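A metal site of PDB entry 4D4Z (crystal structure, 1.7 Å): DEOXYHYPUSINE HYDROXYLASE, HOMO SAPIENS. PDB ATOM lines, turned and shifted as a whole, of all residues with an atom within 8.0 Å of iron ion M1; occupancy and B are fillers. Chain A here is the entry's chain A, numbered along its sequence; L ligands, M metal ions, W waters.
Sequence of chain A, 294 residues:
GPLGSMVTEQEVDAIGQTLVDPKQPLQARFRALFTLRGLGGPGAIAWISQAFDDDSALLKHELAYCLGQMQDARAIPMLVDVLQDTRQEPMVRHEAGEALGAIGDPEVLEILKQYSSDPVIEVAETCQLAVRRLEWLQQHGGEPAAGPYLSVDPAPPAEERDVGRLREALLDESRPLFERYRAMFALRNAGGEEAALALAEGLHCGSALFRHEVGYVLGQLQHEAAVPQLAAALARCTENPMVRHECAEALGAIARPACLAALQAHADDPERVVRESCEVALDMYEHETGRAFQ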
ATOM      1  N   ALA A  57       9.613 -27.886 -26.009  1.00  0.00           N
ATOM      2  CA  ALA A  57       9.793 -26.623 -26.725  1.00  0.00           C
ATOM      3  C   ALA A  57      10.754 -25.681 -25.969  1.00  0.00           C
ATOM      4  O   ALA A  57      11.534 -24.975 -26.596  1.00  0.00           O
ATOM      5  CB  ALA A  57       8.454 -25.903 -26.947  1.00  0.00           C
ATOM      6  N   LEU A  58      10.731 -25.727 -24.625  1.00  0.00           N
ATOM      7  CA  LEU A  58      11.693 -24.952 -23.863  1.00  0.00           C
ATOM      8  C   LEU A  58      13.143 -25.330 -24.191  1.00  0.00           C
ATOM      9  O   LEU A  58      13.968 -24.445 -24.530  1.00  0.00           O
ATOM     10  CB  LEU A  58      11.462 -25.026 -22.357  1.00  0.00           C
ATOM     11  CG  LEU A  58      12.345 -24.144 -21.541  1.00  0.00           C
ATOM     12  CD1 LEU A  58      11.880 -22.726 -21.709  1.00  0.00           C
ATOM     13  CD2 LEU A  58      12.284 -24.503 -20.085  1.00  0.00           C
ATOM     14  N   HIS A  61      14.106 -24.422 -27.928  1.00  0.00           N
ATOM     15  CA  HIS A  61      14.337 -23.010 -28.204  1.00  0.00           C
ATOM     16  C   HIS A  61      15.691 -22.556 -27.602  1.00  0.00           C
ATOM     17  O   HIS A  61      16.376 -21.758 -28.177  1.00  0.00           O
ATOM     18  CB  HIS A  61      13.116 -22.150 -27.850  1.00  0.00           C
ATOM     19  CG  HIS A  61      13.241 -21.287 -26.649  1.00  0.00           C
ATOM     20  ND1 HIS A  61      13.452 -21.773 -25.388  1.00  0.00           N
ATOM     21  CD2 HIS A  61      13.173 -19.948 -26.509  1.00  0.00           C
ATOM     22  CE1 HIS A  61      13.479 -20.788 -24.523  1.00  0.00           C
ATOM     23  NE2 HIS A  61      13.323 -19.662 -25.179  1.00  0.00           N
ATOM     24  N   GLU A  62      16.077 -23.144 -26.465  1.00  0.00           N
ATOM     25  CA  GLU A  62      17.375 -22.811 -25.860  1.00  0.00           C
ATOM     26  C   GLU A  62      18.526 -23.338 -26.761  1.00  0.00           C
ATOM     27  O   GLU A  62      19.596 -22.668 -26.799  1.00  0.00           O
ATOM     28  CB  GLU A  62      17.576 -23.364 -24.497  1.00  0.00           C
ATOM     29  CG  GLU A  62      18.470 -22.519 -23.646  1.00  0.00           C
ATOM     30  CD  GLU A  62      17.740 -21.264 -23.132  1.00  0.00           C
ATOM     31  OE1 GLU A  62      16.709 -20.862 -23.702  1.00  0.00           O
ATOM     32  OE2 GLU A  62      18.146 -20.678 -22.130  1.00  0.00           O
ATOM     33  N   TYR A  65      18.913 -20.576 -29.228  1.00  0.00           N
ATOM     34  CA  TYR A  65      19.475 -19.403 -28.565  1.00  0.00           C
ATOM     35  C   TYR A  65      20.972 -19.579 -28.444  1.00  0.00           C
ATOM     36  O   TYR A  65      21.732 -18.674 -28.839  1.00  0.00           O
ATOM     37  CB  TYR A  65      18.857 -19.168 -27.173  1.00  0.00           C
ATOM     38  CG  TYR A  65      19.501 -18.020 -26.414  1.00  0.00           C
ATOM     39  CD1 TYR A  65      19.164 -16.684 -26.705  1.00  0.00           C
ATOM     40  CD2 TYR A  65      20.424 -18.276 -25.423  1.00  0.00           C
ATOM     41  CE1 TYR A  65      19.720 -15.658 -25.974  1.00  0.00           C
ATOM     42  CE2 TYR A  65      20.959 -17.236 -24.710  1.00  0.00           C
ATOM     43  CZ  TYR A  65      20.596 -15.977 -24.978  1.00  0.00           C
ATOM     44  OH  TYR A  65      21.219 -14.939 -24.244  1.00  0.00           O
ATOM     45  N   MET A  91       7.705 -20.478 -30.754  1.00  0.00           N
ATOM     46  CA  MET A  91       8.834 -19.935 -29.991  1.00  0.00           C
ATOM     47  C   MET A  91      10.151 -20.573 -30.441  1.00  0.00           C
ATOM     48  O   MET A  91      11.190 -19.914 -30.297  1.00  0.00           O
ATOM     49  CB  MET A  91       8.756 -20.053 -28.458  1.00  0.00           C
ATOM     50  CG  MET A  91       8.780 -21.483 -27.911  1.00  0.00           C
ATOM     51  SD  MET A  91       8.500 -21.507 -26.126  1.00  0.00           S
ATOM     52  CE  MET A  91      10.034 -21.085 -25.261  1.00  0.00           C
ATOM     53  N   HIS A  94      10.946 -18.862 -33.867  1.00  0.00           N
ATOM     54  CA  HIS A  94      11.402 -17.527 -33.558  1.00  0.00           C
ATOM     55  C   HIS A  94      12.869 -17.567 -33.087  1.00  0.00           C
ATOM     56  O   HIS A  94      13.679 -16.771 -33.527  1.00  0.00           O
ATOM     57  CB  HIS A  94      10.480 -16.840 -32.468  1.00  0.00           C
ATOM     58  CG  HIS A  94      11.242 -16.150 -31.375  1.00  0.00           C
ATOM     59  ND1 HIS A  94      11.996 -15.004 -31.552  1.00  0.00           N
ATOM     60  CD2 HIS A  94      11.439 -16.524 -30.090  1.00  0.00           C
ATOM     61  CE1 HIS A  94      12.589 -14.693 -30.409  1.00  0.00           C
ATOM     62  NE2 HIS A  94      12.289 -15.605 -29.519  1.00  0.00           N
ATOM     63  N   GLU A  95      13.193 -18.491 -32.207  1.00  0.00           N
ATOM     64  CA  GLU A  95      14.513 -18.440 -31.607  1.00  0.00           C
ATOM     65  C   GLU A  95      15.592 -18.759 -32.691  1.00  0.00           C
ATOM     66  O   GLU A  95      16.649 -18.204 -32.742  1.00  0.00           O
ATOM     67  CB  GLU A  95      14.607 -19.377 -30.401  1.00  0.00           C
ATOM     68  CG  GLU A  95      15.631 -18.881 -29.401  1.00  0.00           C
ATOM     69  CD  GLU A  95      15.257 -17.550 -28.726  1.00  0.00           C
ATOM     70  OE1 GLU A  95      14.089 -17.401 -28.245  1.00  0.00           O
ATOM     71  OE2 GLU A  95      16.100 -16.593 -28.814  1.00  0.00           O
ATOM     72  N   GLU A  98      15.970 -15.594 -34.869  1.00  0.00           N
ATOM     73  CA  GLU A  98      16.754 -14.629 -34.122  1.00  0.00           C
ATOM     74  C   GLU A  98      18.261 -15.047 -34.177  1.00  0.00           C
ATOM     75  O   GLU A  98      19.132 -14.148 -34.318  1.00  0.00           O
ATOM     76  CB  GLU A  98      16.267 -14.502 -32.654  1.00  0.00           C
ATOM     77  CG  GLU A  98      17.083 -13.446 -31.885  1.00  0.00           C
ATOM     78  CD  GLU A  98      16.628 -13.064 -30.490  1.00  0.00           C
ATOM     79  OE1 GLU A  98      15.433 -12.949 -30.183  1.00  0.00           O
ATOM     80  OE2 GLU A  98      17.550 -12.736 -29.702  1.00  0.00           O
ATOM     81  N   HIS A 212       7.878 -10.562 -24.662  1.00  0.00           N
ATOM     82  CA  HIS A 212       8.864 -11.574 -24.238  1.00  0.00           C
ATOM     83  C   HIS A 212      10.247 -11.007 -24.179  1.00  0.00           C
ATOM     84  O   HIS A 212      11.042 -11.412 -23.300  1.00  0.00           O
ATOM     85  CB  HIS A 212       8.700 -12.845 -25.126  1.00  0.00           C
ATOM     86  CG  HIS A 212       9.899 -13.257 -25.940  1.00  0.00           C
ATOM     87  ND1 HIS A 212      10.350 -12.577 -27.052  1.00  0.00           N
ATOM     88  CD2 HIS A 212      10.718 -14.352 -25.820  1.00  0.00           C
ATOM     89  CE1 HIS A 212      11.414 -13.203 -27.543  1.00  0.00           C
ATOM     90  NE2 HIS A 212      11.629 -14.300 -26.840  1.00  0.00           N
ATOM     91  N   GLU A 213      10.612 -10.121 -25.100  1.00  0.00           N
ATOM     92  CA  GLU A 213      11.949  -9.483 -25.061  1.00  0.00           C
ATOM     93  C   GLU A 213      12.114  -8.619 -23.799  1.00  0.00           C
ATOM     94  O   GLU A 213      13.178  -8.609 -23.165  1.00  0.00           O
ATOM     95  CB  GLU A 213      12.252  -8.722 -26.331  1.00  0.00           C
ATOM     96  CG  GLU A 213      13.728  -8.485 -26.482  1.00  0.00           C
ATOM     97  CD  GLU A 213      14.525  -9.692 -26.888  1.00  0.00           C
ATOM     98  OE1 GLU A 213      13.987 -10.580 -27.498  1.00  0.00           O
ATOM     99  OE2 GLU A 213      15.728  -9.840 -26.518  1.00  0.00           O
ATOM    100  N   TYR A 216      12.883 -10.986 -21.042  1.00  0.00           N
ATOM    101  CA  TYR A 216      14.297 -11.415 -21.144  1.00  0.00           C
ATOM    102  C   TYR A 216      15.238 -10.339 -20.581  1.00  0.00           C
ATOM    103  O   TYR A 216      16.116 -10.657 -19.750  1.00  0.00           O
ATOM    104  CB  TYR A 216      14.607 -11.662 -22.590  1.00  0.00           C
ATOM    105  CG  TYR A 216      16.068 -11.863 -22.885  1.00  0.00           C
ATOM    106  CD1 TYR A 216      16.653 -13.066 -22.668  1.00  0.00           C
ATOM    107  CD2 TYR A 216      16.803 -10.905 -23.552  1.00  0.00           C
ATOM    108  CE1 TYR A 216      18.010 -13.313 -23.003  1.00  0.00           C
ATOM    109  CE2 TYR A 216      18.164 -11.132 -23.868  1.00  0.00           C
ATOM    110  CZ  TYR A 216      18.732 -12.342 -23.589  1.00  0.00           C
ATOM    111  OH  TYR A 216      20.068 -12.541 -24.019  1.00  0.00           O
ATOM    112  N   PRO A 241       2.334 -18.211 -24.315  1.00  0.00           N
ATOM    113  CA  PRO A 241       3.222 -18.987 -23.451  1.00  0.00           C
ATOM    114  C   PRO A 241       4.636 -18.519 -23.525  1.00  0.00           C
ATOM    115  O   PRO A 241       5.366 -18.673 -22.537  1.00  0.00           O
ATOM    116  CB  PRO A 241       3.093 -20.423 -23.966  1.00  0.00           C
ATOM    117  CG  PRO A 241       1.715 -20.445 -24.530  1.00  0.00           C
ATOM    118  CD  PRO A 241       1.517 -19.104 -25.178  1.00  0.00           C
ATOM    119  N   MET A 242       5.069 -17.966 -24.678  1.00  0.00           N
ATOM    120  CA  MET A 242       6.422 -17.453 -24.812  1.00  0.00           C
ATOM    121  C   MET A 242       6.702 -16.300 -23.833  1.00  0.00           C
ATOM    122  O   MET A 242       7.799 -16.183 -23.286  1.00  0.00           O
ATOM    123  CB  MET A 242       6.714 -16.976 -26.231  1.00  0.00           C
ATOM    124  CG  MET A 242       8.161 -16.618 -26.478  1.00  0.00           C
ATOM    125  SD  MET A 242       8.369 -16.013 -28.170  1.00  0.00           S
ATOM    126  CE  MET A 242       7.294 -17.107 -29.041  1.00  0.00           C
ATOM    127  N   VAL A 243       5.743 -15.432 -23.656  1.00  0.00           N
ATOM    128  CA  VAL A 243       5.897 -14.360 -22.737  1.00  0.00           C
ATOM    129  C   VAL A 243       5.907 -14.844 -21.284  1.00  0.00           C
ATOM    130  O   VAL A 243       6.737 -14.429 -20.491  1.00  0.00           O
ATOM    131  CB  VAL A 243       4.740 -13.318 -22.913  1.00  0.00           C
ATOM    132  CG1 VAL A 243       4.876 -12.230 -21.883  1.00  0.00           C
ATOM    133  CG2 VAL A 243       4.776 -12.697 -24.342  1.00  0.00           C
ATOM    134  N   HIS A 245       6.783 -17.753 -20.163  1.00  0.00           N
ATOM    135  CA  HIS A 245       8.066 -18.463 -19.936  1.00  0.00           C
ATOM    136  C   HIS A 245       9.174 -17.506 -19.652  1.00  0.00           C
ATOM    137  O   HIS A 245       9.953 -17.656 -18.711  1.00  0.00           O
ATOM    138  CB  HIS A 245       8.305 -19.386 -21.147  1.00  0.00           C
ATOM    139  CG  HIS A 245       9.619 -19.170 -21.779  1.00  0.00           C
ATOM    140  ND1 HIS A 245      10.771 -19.674 -21.186  1.00  0.00           N
ATOM    141  CD2 HIS A 245      10.006 -18.531 -22.895  1.00  0.00           C
ATOM    142  CE1 HIS A 245      11.822 -19.313 -21.910  1.00  0.00           C
ATOM    143  NE2 HIS A 245      11.371 -18.637 -22.956  1.00  0.00           N
ATOM    144  N   GLU A 246       9.295 -16.400 -20.399  1.00  0.00           N
ATOM    145  CA  GLU A 246      10.368 -15.505 -20.247  1.00  0.00           C
ATOM    146  C   GLU A 246      10.249 -14.778 -18.908  1.00  0.00           C
ATOM    147  O   GLU A 246      11.248 -14.514 -18.188  1.00  0.00           O
ATOM    148  CB  GLU A 246      10.423 -14.574 -21.474  1.00  0.00           C
ATOM    149  CG  GLU A 246      11.756 -14.175 -21.887  1.00  0.00           C
ATOM    150  CD  GLU A 246      12.591 -15.299 -22.459  1.00  0.00           C
ATOM    151  OE1 GLU A 246      12.197 -15.984 -23.445  1.00  0.00           O
ATOM    152  OE2 GLU A 246      13.665 -15.472 -21.846  1.00  0.00           O
ATOM    153  N   CYS A 247       9.007 -14.479 -18.511  1.00  0.00           N
ATOM    154  CA  CYS A 247       8.839 -13.801 -17.223  1.00  0.00           C
ATOM    155  C   CYS A 247       9.179 -14.762 -16.044  1.00  0.00           C
ATOM    156  O   CYS A 247       9.753 -14.315 -15.076  1.00  0.00           O
ATOM    157  CB  CYS A 247       7.420 -13.297 -17.062  1.00  0.00           C
ATOM    158  SG  CYS A 247       7.104 -11.914 -18.236  1.00  0.00           S
ATOM    159  N   GLU A 249      11.420 -17.188 -16.155  1.00  0.00           N
ATOM    160  CA  GLU A 249      12.890 -17.234 -16.120  1.00  0.00           C
ATOM    161  C   GLU A 249      13.508 -15.962 -15.510  1.00  0.00           C
ATOM    162  O   GLU A 249      14.426 -16.018 -14.660  1.00  0.00           O
ATOM    163  CB  GLU A 249      13.477 -17.531 -17.491  1.00  0.00           C
ATOM    164  CG  GLU A 249      13.013 -18.900 -17.917  1.00  0.00           C
ATOM    165  CD  GLU A 249      13.918 -19.599 -18.826  1.00  0.00           C
ATOM    166  OE1 GLU A 249      14.989 -19.013 -19.138  1.00  0.00           O
ATOM    167  OE2 GLU A 249      13.460 -20.727 -19.172  1.00  0.00           O
ATOM    168  N   VAL A 273       5.456 -25.435 -21.478  1.00  0.00           N
ATOM    169  CA  VAL A 273       6.593 -24.508 -21.498  1.00  0.00           C
ATOM    170  C   VAL A 273       6.641 -23.658 -20.233  1.00  0.00           C
ATOM    171  O   VAL A 273       7.719 -23.347 -19.725  1.00  0.00           O
ATOM    172  CB  VAL A 273       6.691 -23.676 -22.788  1.00  0.00           C
ATOM    173  CG1 VAL A 273       5.693 -22.608 -22.826  1.00  0.00           C
ATOM    174  CG2 VAL A 273       8.030 -22.942 -22.837  1.00  0.00           C
ATOM    175  N   SER A 277       9.678 -23.855 -17.477  1.00  0.00           N
ATOM    176  CA  SER A 277      10.377 -22.665 -17.132  1.00  0.00           C
ATOM    177  C   SER A 277      10.387 -22.443 -15.599  1.00  0.00           C
ATOM    178  O   SER A 277      11.402 -22.064 -15.031  1.00  0.00           O
ATOM    179  CB  SER A 277       9.804 -21.427 -17.746  1.00  0.00           C
ATOM    180  OG  SER A 277       9.937 -21.462 -19.158  1.00  0.00           O
HETATM  181  C1  LIG L   1      16.469 -13.420 -26.512  1.00  0.00           C
HETATM  182  O1  LIG L   1      16.666 -12.158 -27.283  1.00  0.00           O
HETATM  183  C2  LIG L   1      15.064 -13.966 -26.526  1.00  0.00           C
HETATM  184  O2  LIG L   1      14.647 -14.565 -27.819  1.00  0.00           O
HETATM  185  C3  LIG L   1      14.882 -15.006 -25.401  1.00  0.00           C
HETATM  186  O3  LIG L   1      14.097 -16.130 -25.690  1.00  0.00           O
HETATM  187  O1  LG2 L   2      11.778 -17.209 -26.396  1.00  0.00           O
HETATM  188 FE    FE M   1      12.761 -17.609 -24.453  1.00  0.00          FE
HETATM  189 FE    FE M   2      12.969 -15.905 -27.438  1.00  0.00          FE
HETATM  190  O   HOH W   1      14.282 -17.790 -23.043  1.00  0.00           O
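A ring nitrogen (ND1) of His 61 is in hydrogen-bond range of the backbone carbonyl oxygen (O) of Leu 58 (2.9 Å).
The side-chain hydroxyl of Ser 277 sits at hydrogen-bond distance from a ring nitrogen (ND1) of His 245 (2.8 Å).
Of the 21 residues printed, 3 come within 4 Å of iron ion M1.
The nearest printed residue that does not touch iron ion M1 is Glu 95 (4.02 Å).
Iron ion M1 is bound by OE1 of Glu 246 (2.0 Å), water W1 (2.1 Å), O1 of LG2 L2 (2.2 Å), NE2 of His 61 (2.2 Å), NE2 of His 245 (2.3 Å) and O3 of LIG L1 (2.3 Å).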
